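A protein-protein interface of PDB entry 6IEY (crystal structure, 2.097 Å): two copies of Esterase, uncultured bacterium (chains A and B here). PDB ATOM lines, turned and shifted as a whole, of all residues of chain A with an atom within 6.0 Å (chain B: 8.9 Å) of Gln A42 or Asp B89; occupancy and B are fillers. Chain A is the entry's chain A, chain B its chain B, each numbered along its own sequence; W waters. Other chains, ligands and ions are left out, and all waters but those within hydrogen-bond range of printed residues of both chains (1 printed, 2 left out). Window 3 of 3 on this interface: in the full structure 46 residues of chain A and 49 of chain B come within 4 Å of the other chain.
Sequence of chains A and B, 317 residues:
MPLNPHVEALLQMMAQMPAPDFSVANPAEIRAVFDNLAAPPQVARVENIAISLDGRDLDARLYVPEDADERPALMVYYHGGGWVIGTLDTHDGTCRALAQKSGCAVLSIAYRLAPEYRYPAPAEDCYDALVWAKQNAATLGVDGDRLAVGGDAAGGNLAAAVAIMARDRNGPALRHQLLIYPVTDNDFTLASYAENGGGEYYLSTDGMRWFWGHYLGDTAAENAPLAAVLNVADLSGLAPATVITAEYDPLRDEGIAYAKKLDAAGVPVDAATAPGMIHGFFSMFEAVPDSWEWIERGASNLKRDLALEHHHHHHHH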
ATOM      1  N   ASP A  35      -7.884  -7.354  20.266  1.00  0.00           N
ATOM      2  CA  ASP A  35      -6.593  -7.620  19.650  1.00  0.00           C
ATOM      3  C   ASP A  35      -6.817  -8.562  18.491  1.00  0.00           C
ATOM      4  O   ASP A  35      -6.112  -8.501  17.477  1.00  0.00           O
ATOM      5  CB  ASP A  35      -5.585  -8.175  20.669  1.00  0.00           C
ATOM      6  CG  ASP A  35      -5.146  -7.104  21.688  1.00  0.00           C
ATOM      7  OD1 ASP A  35      -5.400  -5.913  21.411  1.00  0.00           O
ATOM      8  OD2 ASP A  35      -4.562  -7.425  22.753  1.00  0.00           O
ATOM      9  N   ASN A  36      -7.858  -9.377  18.600  1.00  0.00           N
ATOM     10  CA  ASN A  36      -8.140 -10.344  17.556  1.00  0.00           C
ATOM     11  C   ASN A  36      -9.081  -9.856  16.450  1.00  0.00           C
ATOM     12  O   ASN A  36      -9.368 -10.598  15.527  1.00  0.00           O
ATOM     13  CB  ASN A  36      -8.694 -11.624  18.172  1.00  0.00           C
ATOM     14  CG  ASN A  36      -7.691 -12.755  18.130  1.00  0.00           C
ATOM     15  OD1 ASN A  36      -6.867 -12.823  17.215  1.00  0.00           O
ATOM     16  ND2 ASN A  36      -7.739 -13.644  19.127  1.00  0.00           N
ATOM     17  N   ALA A  39      -6.930  -7.963  12.764  1.00  0.00           N
ATOM     18  CA  ALA A  39      -5.496  -8.158  12.978  1.00  0.00           C
ATOM     19  C   ALA A  39      -5.077  -9.604  12.713  1.00  0.00           C
ATOM     20  O   ALA A  39      -5.852 -10.524  12.960  1.00  0.00           O
ATOM     21  CB  ALA A  39      -5.113  -7.749  14.409  1.00  0.00           C
ATOM     22  N   PRO A  40      -3.842  -9.804  12.218  1.00  0.00           N
ATOM     23  CA  PRO A  40      -3.307 -11.163  12.057  1.00  0.00           C
ATOM     24  C   PRO A  40      -3.182 -11.871  13.406  1.00  0.00           C
ATOM     25  O   PRO A  40      -2.601 -11.298  14.330  1.00  0.00           O
ATOM     26  CB  PRO A  40      -1.920 -10.935  11.432  1.00  0.00           C
ATOM     27  CG  PRO A  40      -1.533  -9.530  11.869  1.00  0.00           C
ATOM     28  CD  PRO A  40      -2.843  -8.765  11.882  1.00  0.00           C
ATOM     29  N   PRO A  41      -3.707 -13.101  13.514  1.00  0.00           N
ATOM     30  CA  PRO A  41      -3.661 -13.875  14.763  1.00  0.00           C
ATOM     31  C   PRO A  41      -2.237 -14.039  15.296  1.00  0.00           C
ATOM     32  O   PRO A  41      -1.290 -14.244  14.520  1.00  0.00           O
ATOM     33  CB  PRO A  41      -4.252 -15.235  14.366  1.00  0.00           C
ATOM     34  CG  PRO A  41      -5.009 -14.985  13.141  1.00  0.00           C
ATOM     35  CD  PRO A  41      -4.304 -13.867  12.413  1.00  0.00           C
ATOM     36  N   GLN A  42      -2.086 -13.940  16.613  1.00  0.00           N
ATOM     37  CA  GLN A  42      -0.769 -13.989  17.229  1.00  0.00           C
ATOM     38  C   GLN A  42      -0.223 -15.405  17.246  1.00  0.00           C
ATOM     39  O   GLN A  42      -0.947 -16.369  17.478  1.00  0.00           O
ATOM     40  CB  GLN A  42      -0.800 -13.420  18.657  1.00  0.00           C
ATOM     41  CG  GLN A  42      -1.253 -11.954  18.742  1.00  0.00           C
ATOM     42  CD  GLN A  42      -0.641 -11.195  19.919  1.00  0.00           C
ATOM     43  OE1 GLN A  42       0.184 -10.291  19.735  1.00  0.00           O
ATOM     44  NE2 GLN A  42      -1.057 -11.546  21.129  1.00  0.00           N
ATOM     45  N   VAL A  43       1.064 -15.532  16.967  1.00  0.00           N
ATOM     46  CA  VAL A  43       1.741 -16.812  17.124  1.00  0.00           C
ATOM     47  C   VAL A  43       3.043 -16.552  17.854  1.00  0.00           C
ATOM     48  O   VAL A  43       3.504 -15.421  17.891  1.00  0.00           O
ATOM     49  CB  VAL A  43       2.014 -17.487  15.789  1.00  0.00           C
ATOM     50  CG1 VAL A  43       0.685 -17.893  15.101  1.00  0.00           C
ATOM     51  CG2 VAL A  43       2.804 -16.567  14.931  1.00  0.00           C
ATOM     52  N   ALA A  44       3.644 -17.587  18.430  1.00  0.00           N
ATOM     53  CA  ALA A  44       4.806 -17.378  19.289  1.00  0.00           C
ATOM     54  C   ALA A  44       6.076 -17.042  18.497  1.00  0.00           C
ATOM     55  O   ALA A  44       6.841 -16.165  18.868  1.00  0.00           O
ATOM     56  CB  ALA A  44       5.027 -18.601  20.154  1.00  0.00           C
ATOM     57  N   PRO A  65       2.920 -21.826  17.000  1.00  0.00           N
ATOM     58  CA  PRO A  65       1.886 -21.102  17.729  1.00  0.00           C
ATOM     59  C   PRO A  65       2.126 -21.148  19.219  1.00  0.00           C
ATOM     60  O   PRO A  65       2.925 -21.954  19.716  1.00  0.00           O
ATOM     61  CB  PRO A  65       0.607 -21.850  17.354  1.00  0.00           C
ATOM     62  CG  PRO A  65       1.065 -23.239  17.108  1.00  0.00           C
ATOM     63  CD  PRO A  65       2.471 -23.162  16.578  1.00  0.00           C
ATOM     64  N   GLU A  66       1.432 -20.266  19.921  1.00  0.00           N
ATOM     65  CA  GLU A  66       1.443 -20.274  21.375  1.00  0.00           C
ATOM     66  C   GLU A  66       1.017 -21.655  21.880  1.00  0.00           C
ATOM     67  O   GLU A  66       0.129 -22.291  21.306  1.00  0.00           O
ATOM     68  CB  GLU A  66       0.519 -19.175  21.915  1.00  0.00           C
ATOM     69  CG  GLU A  66       1.013 -18.530  23.213  1.00  0.00           C
ATOM     70  CD  GLU A  66       2.401 -17.924  23.070  1.00  0.00           C
ATOM     71  OE1 GLU A  66       2.619 -17.168  22.096  1.00  0.00           O
ATOM     72  OE2 GLU A  66       3.273 -18.216  23.922  1.00  0.00           O
ATOM     73  N   ARG A  96      -1.178 -18.206  10.130  1.00  0.00           N
ATOM     74  CA  ARG A  96      -1.287 -17.867  11.541  1.00  0.00           C
ATOM     75  C   ARG A  96      -2.569 -18.414  12.170  1.00  0.00           C
ATOM     76  O   ARG A  96      -2.533 -18.984  13.252  1.00  0.00           O
ATOM     77  CB  ARG A  96      -1.244 -16.359  11.718  1.00  0.00           C
ATOM     78  CG  ARG A  96       0.099 -15.738  11.393  1.00  0.00           C
ATOM     79  CD  ARG A  96      -0.064 -14.225  11.392  1.00  0.00           C
ATOM     80  NE  ARG A  96       1.213 -13.536  11.296  1.00  0.00           N
ATOM     81  CZ  ARG A  96       1.985 -13.245  12.332  1.00  0.00           C
ATOM     82  NH1 ARG A  96       1.596 -13.548  13.560  1.00  0.00           N
ATOM     83  NH2 ARG A  96       3.144 -12.632  12.141  1.00  0.00           N
ATOM     84  N   GLN A 100      -2.514 -21.302  15.031  1.00  0.00           N
ATOM     85  CA  GLN A 100      -3.103 -20.924  16.312  1.00  0.00           C
ATOM     86  C   GLN A 100      -4.224 -21.873  16.711  1.00  0.00           C
ATOM     87  O   GLN A 100      -4.289 -22.318  17.870  1.00  0.00           O
ATOM     88  CB  GLN A 100      -3.615 -19.477  16.260  1.00  0.00           C
ATOM     89  CG  GLN A 100      -4.400 -19.041  17.494  1.00  0.00           C
ATOM     90  CD  GLN A 100      -5.072 -17.675  17.325  1.00  0.00           C
ATOM     91  OE1 GLN A 100      -6.281 -17.583  17.063  1.00  0.00           O
ATOM     92  NE2 GLN A 100      -4.292 -16.606  17.496  1.00  0.00           N
ATOM     93  N   PRO B  40      -0.075  -7.507   3.527  1.00  0.00           N
ATOM     94  CA  PRO B  40       0.289  -6.250   4.202  1.00  0.00           C
ATOM     95  C   PRO B  40       1.342  -5.498   3.387  1.00  0.00           C
ATOM     96  O   PRO B  40       2.002  -6.105   2.538  1.00  0.00           O
ATOM     97  CB  PRO B  40       0.832  -6.717   5.553  1.00  0.00           C
ATOM     98  CG  PRO B  40       1.193  -8.148   5.361  1.00  0.00           C
ATOM     99  CD  PRO B  40       0.237  -8.690   4.346  1.00  0.00           C
ATOM    100  N   VAL B  46      11.569  -7.880   8.215  1.00  0.00           N
ATOM    101  CA  VAL B  46      10.909  -7.724   9.498  1.00  0.00           C
ATOM    102  C   VAL B  46      11.577  -8.633  10.512  1.00  0.00           C
ATOM    103  O   VAL B  46      11.616  -9.843  10.336  1.00  0.00           O
ATOM    104  CB  VAL B  46       9.413  -8.053   9.427  1.00  0.00           C
ATOM    105  CG1 VAL B  46       8.737  -7.697  10.727  1.00  0.00           C
ATOM    106  CG2 VAL B  46       8.765  -7.302   8.296  1.00  0.00           C
ATOM    107  N   ASN B  48      11.813  -9.913  14.457  1.00  0.00           N
ATOM    108  CA  ASN B  48      11.278 -10.004  15.801  1.00  0.00           C
ATOM    109  C   ASN B  48      12.433  -9.878  16.764  1.00  0.00           C
ATOM    110  O   ASN B  48      13.354 -10.686  16.759  1.00  0.00           O
ATOM    111  CB  ASN B  48      10.521 -11.320  16.015  1.00  0.00           C
ATOM    112  CG  ASN B  48       9.096 -11.259  15.496  1.00  0.00           C
ATOM    113  OD1 ASN B  48       8.451 -10.212  15.571  1.00  0.00           O
ATOM    114  ND2 ASN B  48       8.591 -12.378  14.977  1.00  0.00           N
ATOM    115  N   ASP B  59       8.990  -7.301  23.925  1.00  0.00           N
ATOM    116  CA  ASP B  59       9.004  -7.696  22.529  1.00  0.00           C
ATOM    117  C   ASP B  59       9.057  -6.450  21.643  1.00  0.00           C
ATOM    118  O   ASP B  59       8.509  -5.408  21.975  1.00  0.00           O
ATOM    119  CB  ASP B  59       7.780  -8.548  22.194  1.00  0.00           C
ATOM    120  CG  ASP B  59       7.891  -9.965  22.723  1.00  0.00           C
ATOM    121  OD1 ASP B  59       9.034 -10.431  22.963  1.00  0.00           O
ATOM    122  OD2 ASP B  59       6.833 -10.610  22.905  1.00  0.00           O
ATOM    123  N   ARG B  61       9.657  -5.181  17.184  1.00  0.00           N
ATOM    124  CA  ARG B  61       9.709  -5.590  15.802  1.00  0.00           C
ATOM    125  C   ARG B  61      10.375  -4.499  15.001  1.00  0.00           C
ATOM    126  O   ARG B  61      10.020  -3.328  15.122  1.00  0.00           O
ATOM    127  CB  ARG B  61       8.303  -5.892  15.293  1.00  0.00           C
ATOM    128  CG  ARG B  61       8.267  -6.739  14.073  1.00  0.00           C
ATOM    129  CD  ARG B  61       6.851  -7.188  13.808  1.00  0.00           C
ATOM    130  NE  ARG B  61       6.414  -8.261  14.691  1.00  0.00           N
ATOM    131  CZ  ARG B  61       5.164  -8.714  14.732  1.00  0.00           C
ATOM    132  NH1 ARG B  61       4.240  -8.162  13.957  1.00  0.00           N
ATOM    133  NH2 ARG B  61       4.835  -9.712  15.542  1.00  0.00           N
ATOM    134  N   TYR B  63      11.194  -3.048  11.274  1.00  0.00           N
ATOM    135  CA  TYR B  63      10.756  -3.088   9.896  1.00  0.00           C
ATOM    136  C   TYR B  63      11.787  -2.362   9.084  1.00  0.00           C
ATOM    137  O   TYR B  63      12.076  -1.204   9.363  1.00  0.00           O
ATOM    138  CB  TYR B  63       9.382  -2.418   9.715  1.00  0.00           C
ATOM    139  CG  TYR B  63       8.300  -3.023  10.559  1.00  0.00           C
ATOM    140  CD1 TYR B  63       8.102  -2.604  11.874  1.00  0.00           C
ATOM    141  CD2 TYR B  63       7.482  -4.011  10.051  1.00  0.00           C
ATOM    142  CE1 TYR B  63       7.137  -3.156  12.649  1.00  0.00           C
ATOM    143  CE2 TYR B  63       6.495  -4.569  10.823  1.00  0.00           C
ATOM    144  CZ  TYR B  63       6.333  -4.137  12.125  1.00  0.00           C
ATOM    145  OH  TYR B  63       5.365  -4.697  12.898  1.00  0.00           O
ATOM    146  N   HIS B  79       2.597   1.552  19.710  1.00  0.00           N
ATOM    147  CA  HIS B  79       1.239   1.302  19.251  1.00  0.00           C
ATOM    148  C   HIS B  79       0.224   1.996  20.159  1.00  0.00           C
ATOM    149  O   HIS B  79       0.506   2.276  21.321  1.00  0.00           O
ATOM    150  CB  HIS B  79       0.945  -0.207  19.194  1.00  0.00           C
ATOM    151  CG  HIS B  79       0.934  -0.872  20.539  1.00  0.00           C
ATOM    152  ND1 HIS B  79      -0.145  -0.799  21.400  1.00  0.00           N
ATOM    153  CD2 HIS B  79       1.870  -1.619  21.171  1.00  0.00           C
ATOM    154  CE1 HIS B  79       0.134  -1.465  22.504  1.00  0.00           C
ATOM    155  NE2 HIS B  79       1.348  -1.976  22.390  1.00  0.00           N
ATOM    156  N   GLY B  86      -3.787  -3.479  22.428  1.00  0.00           N
ATOM    157  CA  GLY B  86      -2.857  -3.240  21.340  1.00  0.00           C
ATOM    158  C   GLY B  86      -1.673  -4.189  21.441  1.00  0.00           C
ATOM    159  O   GLY B  86      -1.212  -4.508  22.545  1.00  0.00           O
ATOM    160  N   THR B  87      -1.184  -4.652  20.290  1.00  0.00           N
ATOM    161  CA  THR B  87      -0.021  -5.526  20.243  1.00  0.00           C
ATOM    162  C   THR B  87       0.848  -5.178  19.033  1.00  0.00           C
ATOM    163  O   THR B  87       0.503  -4.312  18.213  1.00  0.00           O
ATOM    164  CB  THR B  87      -0.411  -7.030  20.149  1.00  0.00           C
ATOM    165  OG1 THR B  87      -0.949  -7.291  18.848  1.00  0.00           O
ATOM    166  CG2 THR B  87      -1.447  -7.431  21.210  1.00  0.00           C
ATOM    167  N   LEU B  88       1.966  -5.878  18.909  1.00  0.00           N
ATOM    168  CA  LEU B  88       2.798  -5.742  17.730  1.00  0.00           C
ATOM    169  C   LEU B  88       1.986  -6.148  16.505  1.00  0.00           C
ATOM    170  O   LEU B  88       2.066  -5.497  15.487  1.00  0.00           O
ATOM    171  CB  LEU B  88       4.075  -6.576  17.862  1.00  0.00           C
ATOM    172  CG  LEU B  88       5.077  -6.105  18.925  1.00  0.00           C
ATOM    173  CD1 LEU B  88       6.410  -6.823  18.771  1.00  0.00           C
ATOM    174  CD2 LEU B  88       5.276  -4.591  18.870  1.00  0.00           C
ATOM    175  N   ASP B  89       1.161  -7.183  16.625  1.00  0.00           N
ATOM    176  CA  ASP B  89       0.367  -7.650  15.484  1.00  0.00           C
ATOM    177  C   ASP B  89      -0.753  -6.688  15.030  1.00  0.00           C
ATOM    178  O   ASP B  89      -0.953  -6.515  13.830  1.00  0.00           O
ATOM    179  CB  ASP B  89      -0.219  -9.031  15.793  1.00  0.00           C
ATOM    180  CG  ASP B  89       0.858 -10.123  15.828  1.00  0.00           C
ATOM    181  OD1 ASP B  89       1.871 -10.019  15.099  1.00  0.00           O
ATOM    182  OD2 ASP B  89       0.703 -11.081  16.609  1.00  0.00           O
ATOM    183  N   THR B  90      -1.456  -6.050  15.963  1.00  0.00           N
ATOM    184  CA  THR B  90      -2.498  -5.103  15.579  1.00  0.00           C
ATOM    185  C   THR B  90      -1.920  -3.888  14.831  1.00  0.00           C
ATOM    186  O   THR B  90      -2.595  -3.235  14.038  1.00  0.00           O
ATOM    187  CB  THR B  90      -3.302  -4.600  16.806  1.00  0.00           C
ATOM    188  OG1 THR B  90      -2.477  -3.736  17.607  1.00  0.00           O
ATOM    189  CG2 THR B  90      -3.820  -5.780  17.647  1.00  0.00           C
ATOM    190  N   HIS B  91      -0.667  -3.564  15.073  1.00  0.00           N
ATOM    191  CA  HIS B  91      -0.139  -2.404  14.379  1.00  0.00           C
ATOM    192  C   HIS B  91       0.921  -2.747  13.386  1.00  0.00           C
ATOM    193  O   HIS B  91       1.616  -1.863  12.909  1.00  0.00           O
ATOM    194  CB  HIS B  91       0.377  -1.397  15.380  1.00  0.00           C
ATOM    195  CG  HIS B  91      -0.719  -0.669  16.078  1.00  0.00           C
ATOM    196  ND1 HIS B  91      -1.710  -1.324  16.776  1.00  0.00           N
ATOM    197  CD2 HIS B  91      -1.005   0.651  16.158  1.00  0.00           C
ATOM    198  CE1 HIS B  91      -2.546  -0.436  17.280  1.00  0.00           C
ATOM    199  NE2 HIS B  91      -2.140   0.770  16.923  1.00  0.00           N
ATOM    200  N   ASP B  92       1.015  -4.028  13.042  1.00  0.00           N
ATOM    201  CA  ASP B  92       2.027  -4.465  12.103  1.00  0.00           C
ATOM    202  C   ASP B  92       1.840  -3.760  10.742  1.00  0.00           C
ATOM    203  O   ASP B  92       2.802  -3.321  10.124  1.00  0.00           O
ATOM    204  CB  ASP B  92       1.983  -5.983  11.952  1.00  0.00           C
ATOM    205  CG  ASP B  92       3.172  -6.518  11.181  1.00  0.00           C
ATOM    206  OD1 ASP B  92       4.210  -6.808  11.811  1.00  0.00           O
ATOM    207  OD2 ASP B  92       3.081  -6.625   9.942  1.00  0.00           O
ATOM    208  N   GLY B  93       0.598  -3.625  10.291  1.00  0.00           N
ATOM    209  CA  GLY B  93       0.311  -2.957   9.019  1.00  0.00           C
ATOM    210  C   GLY B  93       0.697  -1.479   8.977  1.00  0.00           C
ATOM    211  O   GLY B  93       1.305  -0.985   8.007  1.00  0.00           O
ATOM    212  N   THR B  94       0.351  -0.775  10.048  1.00  0.00           N
ATOM    213  CA  THR B  94       0.657   0.649  10.202  1.00  0.00           C
ATOM    214  C   THR B  94       2.160   0.919  10.209  1.00  0.00           C
ATOM    215  O   THR B  94       2.640   1.860   9.561  1.00  0.00           O
ATOM    216  CB  THR B  94       0.034   1.190  11.506  1.00  0.00           C
ATOM    217  OG1 THR B  94      -1.365   0.874  11.515  1.00  0.00           O
ATOM    218  CG2 THR B  94       0.203   2.690  11.604  1.00  0.00           C
ATOM    219  N   CYS B  95       2.908   0.111  10.957  1.00  0.00           N
ATOM    220  CA  CYS B  95       4.353   0.246  10.963  1.00  0.00           C
ATOM    221  C   CYS B  95       4.950  -0.032   9.582  1.00  0.00           C
ATOM    222  O   CYS B  95       5.860   0.672   9.152  1.00  0.00           O
ATOM    223  CB  CYS B  95       4.973  -0.685  12.011  1.00  0.00           C
ATOM    224  SG  CYS B  95       4.449  -0.270  13.682  1.00  0.00           S
ATOM    225  N   ARG B  96       4.448  -1.047   8.885  1.00  0.00           N
ATOM    226  CA  ARG B  96       4.968  -1.355   7.549  1.00  0.00           C
ATOM    227  C   ARG B  96       4.685  -0.204   6.595  1.00  0.00           C
ATOM    228  O   ARG B  96       5.560   0.205   5.813  1.00  0.00           O
ATOM    229  CB  ARG B  96       4.352  -2.639   6.991  1.00  0.00           C
ATOM    230  CG  ARG B  96       4.862  -3.945   7.581  1.00  0.00           C
ATOM    231  CD  ARG B  96       3.870  -5.041   7.228  1.00  0.00           C
ATOM    232  NE  ARG B  96       4.350  -6.382   7.509  1.00  0.00           N
ATOM    233  CZ  ARG B  96       5.054  -7.108   6.647  1.00  0.00           C
ATOM    234  NH1 ARG B  96       5.369  -6.600   5.456  1.00  0.00           N
ATOM    235  NH2 ARG B  96       5.443  -8.336   6.974  1.00  0.00           N
ATOM    236  N   SER B 108       8.978  -1.083  16.396  1.00  0.00           N
ATOM    237  CA  SER B 108       7.726  -1.054  17.148  1.00  0.00           C
ATOM    238  C   SER B 108       7.888  -1.737  18.523  1.00  0.00           C
ATOM    239  O   SER B 108       8.355  -2.877  18.605  1.00  0.00           O
ATOM    240  CB  SER B 108       6.613  -1.723  16.323  1.00  0.00           C
ATOM    241  OG  SER B 108       5.348  -1.651  16.962  1.00  0.00           O
ATOM    242  N   ILE B 109       7.508  -1.038  19.595  1.00  0.00           N
ATOM    243  CA  ILE B 109       7.720  -1.534  20.955  1.00  0.00           C
ATOM    244  C   ILE B 109       6.444  -2.052  21.632  1.00  0.00           C
ATOM    245  O   ILE B 109       5.431  -1.353  21.716  1.00  0.00           O
ATOM    246  CB  ILE B 109       8.304  -0.446  21.881  1.00  0.00           C
ATOM    247  CG1 ILE B 109       9.472   0.284  21.222  1.00  0.00           C
ATOM    248  CG2 ILE B 109       8.678  -1.045  23.242  1.00  0.00           C
ATOM    249  CD1 ILE B 109      10.630  -0.618  20.856  1.00  0.00           C
ATOM    250  N   ALA B 110       6.497  -3.271  22.145  1.00  0.00           N
ATOM    251  CA  ALA B 110       5.405  -3.743  22.981  1.00  0.00           C
ATOM    252  C   ALA B 110       5.719  -3.403  24.430  1.00  0.00           C
ATOM    253  O   ALA B 110       6.266  -4.217  25.169  1.00  0.00           O
ATOM    254  CB  ALA B 110       5.179  -5.241  22.798  1.00  0.00           C
ATOM    255  N   SER B 283      -4.510   2.949  10.549  1.00  0.00           N
ATOM    256  CA  SER B 283      -4.541   1.496  10.501  1.00  0.00           C
ATOM    257  C   SER B 283      -5.597   0.974   9.534  1.00  0.00           C
ATOM    258  O   SER B 283      -5.688  -0.231   9.334  1.00  0.00           O
ATOM    259  CB  SER B 283      -4.815   0.894  11.891  1.00  0.00           C
ATOM    260  OG  SER B 283      -4.032   1.498  12.895  1.00  0.00           O
HETATM  261  O   HOH W   1      -3.033  -9.229  18.643  1.00  0.00           O
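OD1 of Asp B89 lies within salt-bridge range of NH1 of Arg A96, at 3.9 Å. The side-chain carboxylate of Asp B89 sits close to the side-chain amide oxygen of Gln A42 (3.3 Å). The side-chain hydroxyl (OG1) of Thr B87 lies within hydrogen-bond range of the side-chain amide oxygen (OE1) of Gln A42 (3.3 Å). N of Gly B86 is in hydrogen-bond range of OD1 of Asp A35 (3.1 Å).
The side-chain hydroxyl of Thr B87 lies within hydrogen-bond range of the backbone NH of Asp B89, 3.1 Å away. NH2 of Arg B61 is in salt-bridge range of OD1 of Asp B89. O of Thr B87 is in hydrogen-bond range of OG1 of Thr B90, 3.1 Å away. The side-chain hydroxyl (OG1) of Thr B90 sits at hydrogen-bond distance from a ring nitrogen (ND1) of His B91 (2.7 Å). O of Gln A42 sits at hydrogen-bond distance from NE2 of Gln A100, 3.4 Å away. The guanidinium group (NH1) of Arg A96 is in hydrogen-bond range of the backbone carbonyl oxygen (O) of Pro A41, 3.1 Å away.
Among the printed residues, merely in contact across the chains: Asp A35 with Thr B87 (3.5 Å), Pro A40 with Asp B89 (3.5 Å), Asp A35 with Thr B90 (3.6 Å) and Ala A39 with Thr B90 (3.9 Å).
Printed residues of chain B within 4 Å of Asp A35: Gly B86, Thr B87 and Thr B90. Pro A41 touches none of the printed residues of chain B. Gln A42 touches just these residues of chain B: Thr B87 and Asp B89. Val A43 touches none of the printed residues of chain B. Of the printed residues of chain B, Arg A96 touches Asp B89. Asn B48 touches none of the printed residues of chain A. Of the printed residues of chain A, Gly B86 touches Asp A35 (3.1 Å). Asp B89 touches just these residues of chain A: Pro A40 (3.5 Å), Gln A42 (3.0 Å) and Arg A96 (3.9 Å). Ser B108 touches none of the printed residues of chain A. The nearest residue of chain A that does not touch Asp B89 is Pro A41 (4.3 Å).
Hydrophobic or aromatic side chains of chain A within 4 Å of the printed part of chain B: Ala A39 and Pro A40. Among the printed residues, 8 pairs touch across the chains. Among the printed residues, Asp or Glu carboxylates within 4 Å of a Lys or Arg side-chain nitrogen of the other chain: Arg A96 with Asp B89.
2 positions are printed for both chains. Of the 8 pairs that touch across the chains among the printed residues, none has its exchanged pair printed and touching as well.
Water W1 bridges the side-chain hydroxyl of Thr B87 (2.9 Å) and the backbone carbonyl oxygen of Asp A35 (3.4 Å).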
